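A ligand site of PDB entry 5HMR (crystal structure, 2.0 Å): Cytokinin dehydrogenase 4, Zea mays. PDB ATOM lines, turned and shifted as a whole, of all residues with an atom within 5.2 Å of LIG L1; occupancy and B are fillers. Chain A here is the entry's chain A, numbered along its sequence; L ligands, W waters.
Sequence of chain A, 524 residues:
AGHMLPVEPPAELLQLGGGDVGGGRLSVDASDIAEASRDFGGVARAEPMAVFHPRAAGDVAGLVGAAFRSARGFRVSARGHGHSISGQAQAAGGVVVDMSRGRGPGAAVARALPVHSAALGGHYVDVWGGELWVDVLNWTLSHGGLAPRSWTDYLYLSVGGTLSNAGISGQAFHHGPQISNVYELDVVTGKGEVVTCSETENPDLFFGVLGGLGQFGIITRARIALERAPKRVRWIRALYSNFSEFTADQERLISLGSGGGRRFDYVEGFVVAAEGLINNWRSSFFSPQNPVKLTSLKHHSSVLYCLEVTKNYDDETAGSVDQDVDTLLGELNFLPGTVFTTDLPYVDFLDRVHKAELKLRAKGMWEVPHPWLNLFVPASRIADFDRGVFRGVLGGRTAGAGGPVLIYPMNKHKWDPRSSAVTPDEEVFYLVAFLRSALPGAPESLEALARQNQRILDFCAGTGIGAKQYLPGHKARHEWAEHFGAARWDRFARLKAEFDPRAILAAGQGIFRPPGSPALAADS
OD2 of Asp 153 is in hydrogen-bond range of N1 of LIG L1 (2.7 Å).
The backbone carbonyl oxygen (O) of Ile 168 is in hydrogen-bond range of a nitrogen (N7) of LG2 L2.
The backbone NH (N) of Asp 153 lies within hydrogen-bond range of an oxygen (O8) of LG2 L2, at 2.7 Å.
An oxygen (O7) of LG2 L2 lies within hydrogen-bond range of the side-chain hydroxyl (OH) of Tyr 470.
The side-chain amide oxygen (OD1) of Asn 374 lies close to a nitrogen (N4) of LIG L1, 3.3 Å away.
The backbone NH (N) of Ile 168 is in hydrogen-bond range of an oxygen (O7) of LG2 L2, at 2.9 Å.
A nitrogen (N2) of LIG L1 is in hydrogen-bond range of an oxygen (O8) of LG2 L2.
The backbone carbonyl oxygen of Pro 404 is in hydrogen-bond range of the backbone NH of Leu 435, at 2.8 Å.
N of Leu 406 sits at hydrogen-bond distance from O of Ala 433, 2.8 Å away.
The backbone carbonyl oxygen (O) of Asn 374 sits at hydrogen-bond distance from the backbone NH (N) of Tyr 470 (2.9 Å).
Residues that only touch LIG L1: Val 353 (3.6 Å), Trp 366 (3.4 Å), Trp 372 (3.6 Å), Pro 404 (3.97 Å), Leu 406 (3.4 Å), Leu 435 (3.3 Å), Tyr 470 (3.6 Å) and Leu 471 (3.5 Å).
Hydrophobic or aromatic side chains that line LIG L1: Val 353, Trp 366, Trp 372, Pro 404, Leu 406, Leu 435, Tyr 470 and Leu 471.
The nearest printed residue that does not touch LIG L1 is Leu 360 (4.02 Å).
Water W2 lies within hydrogen-bond range of a nitrogen (N4) of LIG L1 (3.1 Å) and the side-chain amide nitrogen (ND2) of Asn 374 (3.2 Å).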
ATOM      1  N   PHE A  40     -20.202 -11.606 -14.478  1.00  0.00           N
ATOM      2  CA  PHE A  40     -19.743 -12.564 -13.465  1.00  0.00           C
ATOM      3  C   PHE A  40     -18.397 -13.234 -13.830  1.00  0.00           C
ATOM      4  O   PHE A  40     -17.602 -13.558 -12.927  1.00  0.00           O
ATOM      5  CB  PHE A  40     -20.847 -13.596 -13.186  1.00  0.00           C
ATOM      6  CG  PHE A  40     -20.575 -14.542 -12.043  1.00  0.00           C
ATOM      7  CD1 PHE A  40     -20.717 -14.133 -10.722  1.00  0.00           C
ATOM      8  CD2 PHE A  40     -20.206 -15.858 -12.290  1.00  0.00           C
ATOM      9  CE1 PHE A  40     -20.541 -15.038  -9.665  1.00  0.00           C
ATOM     10  CE2 PHE A  40     -20.011 -16.765 -11.247  1.00  0.00           C
ATOM     11  CZ  PHE A  40     -20.183 -16.354  -9.935  1.00  0.00           C
ATOM     12  N   ASP A 153     -30.019 -23.473 -10.469  1.00  0.00           N
ATOM     13  CA  ASP A 153     -29.519 -23.615  -9.080  1.00  0.00           C
ATOM     14  C   ASP A 153     -29.508 -22.257  -8.377  1.00  0.00           C
ATOM     15  O   ASP A 153     -29.545 -22.204  -7.153  1.00  0.00           O
ATOM     16  CB  ASP A 153     -28.067 -24.166  -9.077  1.00  0.00           C
ATOM     17  CG  ASP A 153     -27.939 -25.566  -9.664  1.00  0.00           C
ATOM     18  OD1 ASP A 153     -28.935 -26.321  -9.634  1.00  0.00           O
ATOM     19  OD2 ASP A 153     -26.827 -25.908 -10.139  1.00  0.00           O
ATOM     20  N   ILE A 168     -31.261 -24.917 -16.508  1.00  0.00           N
ATOM     21  CA  ILE A 168     -31.170 -26.284 -16.000  1.00  0.00           C
ATOM     22  C   ILE A 168     -30.812 -26.343 -14.527  1.00  0.00           C
ATOM     23  O   ILE A 168     -30.080 -25.502 -14.022  1.00  0.00           O
ATOM     24  CB  ILE A 168     -30.194 -27.160 -16.832  1.00  0.00           C
ATOM     25  CG1 ILE A 168     -28.728 -26.608 -16.774  1.00  0.00           C
ATOM     26  CG2 ILE A 168     -30.718 -27.365 -18.252  1.00  0.00           C
ATOM     27  CD1 ILE A 168     -27.639 -27.455 -17.538  1.00  0.00           C
ATOM     28  N   VAL A 353     -28.202 -21.271  -3.045  1.00  0.00           N
ATOM     29  CA  VAL A 353     -27.001 -20.671  -3.665  1.00  0.00           C
ATOM     30  C   VAL A 353     -26.845 -19.170  -3.281  1.00  0.00           C
ATOM     31  O   VAL A 353     -25.724 -18.712  -3.048  1.00  0.00           O
ATOM     32  CB  VAL A 353     -26.877 -20.991  -5.197  1.00  0.00           C
ATOM     33  CG1 VAL A 353     -25.624 -20.344  -5.819  1.00  0.00           C
ATOM     34  CG2 VAL A 353     -26.855 -22.509  -5.429  1.00  0.00           C
ATOM     35  N   ALA A 356     -24.960 -19.110  -0.056  1.00  0.00           N
ATOM     36  CA  ALA A 356     -23.532 -19.338  -0.292  1.00  0.00           C
ATOM     37  C   ALA A 356     -22.912 -18.018  -0.798  1.00  0.00           C
ATOM     38  O   ALA A 356     -21.792 -17.675  -0.406  1.00  0.00           O
ATOM     39  CB  ALA A 356     -23.333 -20.456  -1.309  1.00  0.00           C
ATOM     40  N   LEU A 360     -19.733 -15.719   0.678  1.00  0.00           N
ATOM     41  CA  LEU A 360     -18.616 -15.412  -0.216  1.00  0.00           C
ATOM     42  C   LEU A 360     -18.365 -13.902  -0.309  1.00  0.00           C
ATOM     43  O   LEU A 360     -17.215 -13.464  -0.256  1.00  0.00           O
ATOM     44  CB  LEU A 360     -18.813 -16.013  -1.620  1.00  0.00           C
ATOM     45  CG  LEU A 360     -18.697 -17.545  -1.745  1.00  0.00           C
ATOM     46  CD1 LEU A 360     -19.423 -18.062  -2.985  1.00  0.00           C
ATOM     47  CD2 LEU A 360     -17.232 -17.996  -1.767  1.00  0.00           C
ATOM     48  N   TRP A 366     -16.576 -13.188  -3.925  1.00  0.00           N
ATOM     49  CA  TRP A 366     -17.653 -13.208  -4.906  1.00  0.00           C
ATOM     50  C   TRP A 366     -17.279 -12.426  -6.145  1.00  0.00           C
ATOM     51  O   TRP A 366     -17.488 -12.914  -7.251  1.00  0.00           O
ATOM     52  CB  TRP A 366     -18.969 -12.673  -4.284  1.00  0.00           C
ATOM     53  CG  TRP A 366     -20.154 -12.764  -5.205  1.00  0.00           C
ATOM     54  CD1 TRP A 366     -20.759 -11.744  -5.876  1.00  0.00           C
ATOM     55  CD2 TRP A 366     -20.872 -13.953  -5.572  1.00  0.00           C
ATOM     56  NE1 TRP A 366     -21.831 -12.210  -6.591  1.00  0.00           N
ATOM     57  CE2 TRP A 366     -21.928 -13.567  -6.427  1.00  0.00           C
ATOM     58  CE3 TRP A 366     -20.746 -15.317  -5.223  1.00  0.00           C
ATOM     59  CZ2 TRP A 366     -22.845 -14.490  -6.956  1.00  0.00           C
ATOM     60  CZ3 TRP A 366     -21.660 -16.227  -5.749  1.00  0.00           C
ATOM     61  CH2 TRP A 366     -22.698 -15.812  -6.589  1.00  0.00           C
ATOM     62  N   TRP A 372     -15.714 -20.147 -15.720  1.00  0.00           N
ATOM     63  CA  TRP A 372     -16.620 -21.293 -15.693  1.00  0.00           C
ATOM     64  C   TRP A 372     -16.735 -21.989 -17.047  1.00  0.00           C
ATOM     65  O   TRP A 372     -16.814 -21.322 -18.090  1.00  0.00           O
ATOM     66  CB  TRP A 372     -17.998 -20.876 -15.131  1.00  0.00           C
ATOM     67  CG  TRP A 372     -17.984 -20.617 -13.649  1.00  0.00           C
ATOM     68  CD1 TRP A 372     -16.897 -20.574 -12.822  1.00  0.00           C
ATOM     69  CD2 TRP A 372     -19.137 -20.381 -12.815  1.00  0.00           C
ATOM     70  NE1 TRP A 372     -17.294 -20.318 -11.531  1.00  0.00           N
ATOM     71  CE2 TRP A 372     -18.665 -20.244 -11.487  1.00  0.00           C
ATOM     72  CE3 TRP A 372     -20.525 -20.328 -13.046  1.00  0.00           C
ATOM     73  CZ2 TRP A 372     -19.525 -20.035 -10.399  1.00  0.00           C
ATOM     74  CZ3 TRP A 372     -21.378 -20.132 -11.976  1.00  0.00           C
ATOM     75  CH2 TRP A 372     -20.885 -19.988 -10.668  1.00  0.00           C
ATOM     76  N   ASN A 374     -18.940 -25.120 -18.935  1.00  0.00           N
ATOM     77  CA  ASN A 374     -20.095 -26.023 -18.873  1.00  0.00           C
ATOM     78  C   ASN A 374     -20.162 -26.886 -20.093  1.00  0.00           C
ATOM     79  O   ASN A 374     -20.252 -26.376 -21.220  1.00  0.00           O
ATOM     80  CB  ASN A 374     -21.407 -25.227 -18.680  1.00  0.00           C
ATOM     81  CG  ASN A 374     -21.378 -24.406 -17.405  1.00  0.00           C
ATOM     82  OD1 ASN A 374     -21.540 -24.924 -16.321  1.00  0.00           O
ATOM     83  ND2 ASN A 374     -21.071 -23.127 -17.505  1.00  0.00           N
ATOM     84  N   PRO A 404     -16.798 -25.601  -6.991  1.00  0.00           N
ATOM     85  CA  PRO A 404     -17.435 -26.898  -7.253  1.00  0.00           C
ATOM     86  C   PRO A 404     -17.364 -27.406  -8.702  1.00  0.00           C
ATOM     87  O   PRO A 404     -17.246 -26.627  -9.647  1.00  0.00           O
ATOM     88  CB  PRO A 404     -18.885 -26.669  -6.828  1.00  0.00           C
ATOM     89  CG  PRO A 404     -19.108 -25.227  -7.005  1.00  0.00           C
ATOM     90  CD  PRO A 404     -17.797 -24.537  -6.776  1.00  0.00           C
ATOM     91  N   LEU A 406     -19.862 -29.628 -10.824  1.00  0.00           N
ATOM     92  CA  LEU A 406     -21.185 -30.276 -10.853  1.00  0.00           C
ATOM     93  C   LEU A 406     -21.243 -31.381 -11.901  1.00  0.00           C
ATOM     94  O   LEU A 406     -20.612 -31.269 -12.956  1.00  0.00           O
ATOM     95  CB  LEU A 406     -22.320 -29.298 -11.158  1.00  0.00           C
ATOM     96  CG  LEU A 406     -22.564 -28.087 -10.278  1.00  0.00           C
ATOM     97  CD1 LEU A 406     -23.808 -27.356 -10.772  1.00  0.00           C
ATOM     98  CD2 LEU A 406     -22.727 -28.475  -8.767  1.00  0.00           C
ATOM     99  N   LEU A 431     -24.622 -32.856 -17.637  1.00  0.00           N
ATOM    100  CA  LEU A 431     -24.021 -31.555 -17.499  1.00  0.00           C
ATOM    101  C   LEU A 431     -22.769 -31.851 -16.661  1.00  0.00           C
ATOM    102  O   LEU A 431     -22.837 -32.563 -15.647  1.00  0.00           O
ATOM    103  CB  LEU A 431     -24.890 -30.522 -16.742  1.00  0.00           C
ATOM    104  CG  LEU A 431     -24.126 -29.254 -16.230  1.00  0.00           C
ATOM    105  CD1 LEU A 431     -23.726 -28.296 -17.387  1.00  0.00           C
ATOM    106  CD2 LEU A 431     -24.949 -28.504 -15.179  1.00  0.00           C
ATOM    107  N   ALA A 433     -20.161 -29.347 -15.012  1.00  0.00           N
ATOM    108  CA  ALA A 433     -19.906 -27.923 -14.777  1.00  0.00           C
ATOM    109  C   ALA A 433     -18.681 -27.659 -13.892  1.00  0.00           C
ATOM    110  O   ALA A 433     -18.684 -28.010 -12.711  1.00  0.00           O
ATOM    111  CB  ALA A 433     -21.142 -27.266 -14.180  1.00  0.00           C
ATOM    112  N   LEU A 435     -16.943 -25.090 -12.016  1.00  0.00           N
ATOM    113  CA  LEU A 435     -17.322 -23.784 -11.457  1.00  0.00           C
ATOM    114  C   LEU A 435     -16.255 -23.252 -10.522  1.00  0.00           C
ATOM    115  O   LEU A 435     -16.516 -23.010  -9.341  1.00  0.00           O
ATOM    116  CB  LEU A 435     -18.703 -23.868 -10.760  1.00  0.00           C
ATOM    117  CG  LEU A 435     -19.834 -24.569 -11.529  1.00  0.00           C
ATOM    118  CD1 LEU A 435     -21.069 -24.675 -10.659  1.00  0.00           C
ATOM    119  CD2 LEU A 435     -20.189 -23.847 -12.833  1.00  0.00           C
ATOM    120  N   TYR A 470     -22.409 -25.821 -23.009  1.00  0.00           N
ATOM    121  CA  TYR A 470     -23.620 -25.115 -22.597  1.00  0.00           C
ATOM    122  C   TYR A 470     -23.102 -23.679 -22.288  1.00  0.00           C
ATOM    123  O   TYR A 470     -21.967 -23.546 -21.802  1.00  0.00           O
ATOM    124  CB  TYR A 470     -24.265 -25.782 -21.363  1.00  0.00           C
ATOM    125  CG  TYR A 470     -25.440 -24.998 -20.791  1.00  0.00           C
ATOM    126  CD1 TYR A 470     -26.504 -24.613 -21.611  1.00  0.00           C
ATOM    127  CD2 TYR A 470     -25.516 -24.708 -19.427  1.00  0.00           C
ATOM    128  CE1 TYR A 470     -27.599 -23.912 -21.088  1.00  0.00           C
ATOM    129  CE2 TYR A 470     -26.632 -24.057 -18.896  1.00  0.00           C
ATOM    130  CZ  TYR A 470     -27.660 -23.648 -19.723  1.00  0.00           C
ATOM    131  OH  TYR A 470     -28.739 -22.966 -19.205  1.00  0.00           O
ATOM    132  N   LEU A 471     -23.868 -22.615 -22.651  1.00  0.00           N
ATOM    133  CA  LEU A 471     -23.424 -21.191 -22.544  1.00  0.00           C
ATOM    134  C   LEU A 471     -22.124 -21.076 -23.395  1.00  0.00           C
ATOM    135  O   LEU A 471     -21.044 -20.758 -22.842  1.00  0.00           O
ATOM    136  CB  LEU A 471     -23.199 -20.740 -21.082  1.00  0.00           C
ATOM    137  CG  LEU A 471     -24.189 -21.230 -20.014  1.00  0.00           C
ATOM    138  CD1 LEU A 471     -23.680 -20.950 -18.634  1.00  0.00           C
ATOM    139  CD2 LEU A 471     -25.537 -20.598 -20.199  1.00  0.00           C
HETATM  140  C1  LIG L   1     -23.641 -24.167  -6.316  1.00  0.00           C
HETATM  141  C2  LIG L   1     -24.260 -24.549  -7.512  1.00  0.00           C
HETATM  142  C3  LIG L   1     -24.199 -23.719  -8.628  1.00  0.00           C
HETATM  143  C4  LIG L   1     -23.530 -22.509  -8.556  1.00  0.00           C
HETATM  144  C5  LIG L   1     -22.918 -22.112  -7.378  1.00  0.00           C
HETATM  145  C6  LIG L   1     -23.009 -22.939  -6.248  1.00  0.00           C
HETATM  146  O1  LIG L   1     -22.373 -20.804  -7.386  1.00  0.00           O
HETATM  147  C7  LIG L   1     -21.242 -20.527  -6.608  1.00  0.00           C
HETATM  148  F1  LIG L   1     -21.585 -20.519  -5.314  1.00  0.00           F
HETATM  149  F2  LIG L   1     -20.800 -19.324  -6.980  1.00  0.00           F
HETATM  150  F3  LIG L   1     -20.301 -21.441  -6.852  1.00  0.00           F
HETATM  151  N1  LIG L   1     -24.767 -24.184  -9.844  1.00  0.00           N
HETATM  152  C8  LIG L   1     -24.466 -23.693 -11.137  1.00  0.00           C
HETATM  153  O2  LIG L   1     -23.714 -22.734 -11.309  1.00  0.00           O
HETATM  154  N2  LIG L   1     -25.029 -24.371 -12.232  1.00  0.00           N
HETATM  155  C9  LIG L   1     -24.750 -23.919 -13.557  1.00  0.00           C
HETATM  156  C10 LIG L   1     -25.218 -24.444 -14.757  1.00  0.00           C
HETATM  157  N3  LIG L   1     -24.782 -23.774 -15.826  1.00  0.00           N
HETATM  158  N4  LIG L   1     -23.963 -22.737 -15.613  1.00  0.00           N
HETATM  159  S1  LIG L   1     -23.744 -22.624 -14.026  1.00  0.00           S
HETATM  160  P1  LG2 L   2     -27.136 -12.158 -18.995  1.00  0.00           P
HETATM  161  O1  LG2 L   2     -25.959 -12.910 -18.500  1.00  0.00           O
HETATM  162  O2  LG2 L   2     -27.230 -10.644 -18.735  1.00  0.00           O
HETATM  163  O3  LG2 L   2     -27.343 -12.267 -20.551  1.00  0.00           O
HETATM  164  C1  LG2 L   2     -27.141 -13.567 -21.163  1.00  0.00           C
HETATM  165  C2  LG2 L   2     -27.384 -13.495 -22.652  1.00  0.00           C
HETATM  166  O4  LG2 L   2     -28.801 -13.349 -22.897  1.00  0.00           O
HETATM  167  C3  LG2 L   2     -26.732 -12.304 -23.359  1.00  0.00           C
HETATM  168  O5  LG2 L   2     -26.420 -12.596 -24.719  1.00  0.00           O
HETATM  169  C4  LG2 L   2     -27.825 -11.223 -23.265  1.00  0.00           C
HETATM  170  O6  LG2 L   2     -27.678 -10.198 -24.227  1.00  0.00           O
HETATM  171  C5  LG2 L   2     -29.082 -12.076 -23.468  1.00  0.00           C
HETATM  172  N1  LG2 L   2     -30.312 -11.566 -22.858  1.00  0.00           N
HETATM  173  C6  LG2 L   2     -30.486 -11.116 -21.579  1.00  0.00           C
HETATM  174  N2  LG2 L   2     -31.729 -10.858 -21.267  1.00  0.00           N
HETATM  175  C7  LG2 L   2     -32.421 -11.120 -22.448  1.00  0.00           C
HETATM  176  C8  LG2 L   2     -33.781 -10.973 -22.809  1.00  0.00           C
HETATM  177  N3  LG2 L   2     -34.695 -10.428 -22.008  1.00  0.00           N
HETATM  178  N4  LG2 L   2     -34.143 -11.348 -24.056  1.00  0.00           N
HETATM  179  C9  LG2 L   2     -33.197 -11.801 -24.891  1.00  0.00           C
HETATM  180  N5  LG2 L   2     -31.882 -11.935 -24.682  1.00  0.00           N
HETATM  181  C10 LG2 L   2     -31.554 -11.575 -23.431  1.00  0.00           C
HETATM  182  N6  LG2 L   2     -27.624 -21.595 -15.690  1.00  0.00           N
HETATM  183  C11 LG2 L   2     -28.386 -22.703 -15.629  1.00  0.00           C
HETATM  184  O7  LG2 L   2     -29.021 -23.107 -16.611  1.00  0.00           O
HETATM  185  N7  LG2 L   2     -28.483 -23.400 -14.443  1.00  0.00           N
HETATM  186  C12 LG2 L   2     -27.901 -23.040 -13.239  1.00  0.00           C
HETATM  187  O8  LG2 L   2     -28.034 -23.762 -12.265  1.00  0.00           O
HETATM  188  C13 LG2 L   2     -27.124 -21.829 -13.303  1.00  0.00           C
HETATM  189  N8  LG2 L   2     -26.576 -21.385 -12.187  1.00  0.00           N
HETATM  190  C14 LG2 L   2     -25.847 -20.200 -12.252  1.00  0.00           C
HETATM  191  C15 LG2 L   2     -25.326 -19.667 -11.078  1.00  0.00           C
HETATM  192  C16 LG2 L   2     -24.603 -18.479 -11.061  1.00  0.00           C
HETATM  193  C17 LG2 L   2     -23.999 -18.006  -9.762  1.00  0.00           C
HETATM  194  C18 LG2 L   2     -24.412 -17.775 -12.280  1.00  0.00           C
HETATM  195  C19 LG2 L   2     -23.627 -16.487 -12.332  1.00  0.00           C
HETATM  196  C20 LG2 L   2     -24.941 -18.298 -13.459  1.00  0.00           C
HETATM  197  C21 LG2 L   2     -25.660 -19.510 -13.474  1.00  0.00           C
HETATM  198  N9  LG2 L   2     -26.223 -20.047 -14.650  1.00  0.00           N
HETATM  199  C22 LG2 L   2     -27.001 -21.180 -14.595  1.00  0.00           C
HETATM  200  C23 LG2 L   2     -25.920 -19.458 -15.976  1.00  0.00           C
HETATM  201  C24 LG2 L   2     -26.996 -18.468 -16.415  1.00  0.00           C
HETATM  202  O9  LG2 L   2     -28.183 -19.164 -16.826  1.00  0.00           O
HETATM  203  C25 LG2 L   2     -26.489 -17.580 -17.552  1.00  0.00           C
HETATM  204  O10 LG2 L   2     -25.457 -16.726 -17.075  1.00  0.00           O
HETATM  205  C26 LG2 L   2     -27.509 -16.760 -18.348  1.00  0.00           C
HETATM  206  O11 LG2 L   2     -26.822 -15.897 -19.247  1.00  0.00           O
HETATM  207  C27 LG2 L   2     -28.517 -15.977 -17.503  1.00  0.00           C
HETATM  208  O12 LG2 L   2     -27.914 -14.960 -16.679  1.00  0.00           O
HETATM  209  P2  LG2 L   2     -28.507 -13.442 -16.785  1.00  0.00           P
HETATM  210  O13 LG2 L   2     -29.975 -13.367 -16.618  1.00  0.00           O
HETATM  211  O14 LG2 L   2     -27.574 -12.650 -15.881  1.00  0.00           O
HETATM  212  O15 LG2 L   2     -28.418 -12.858 -18.255  1.00  0.00           O
HETATM  213  O   HOH W   1     -27.306 -26.730 -12.765  1.00  0.00           O
HETATM  214  O   HOH W   2     -21.918 -20.403 -16.003  1.00  0.00           O
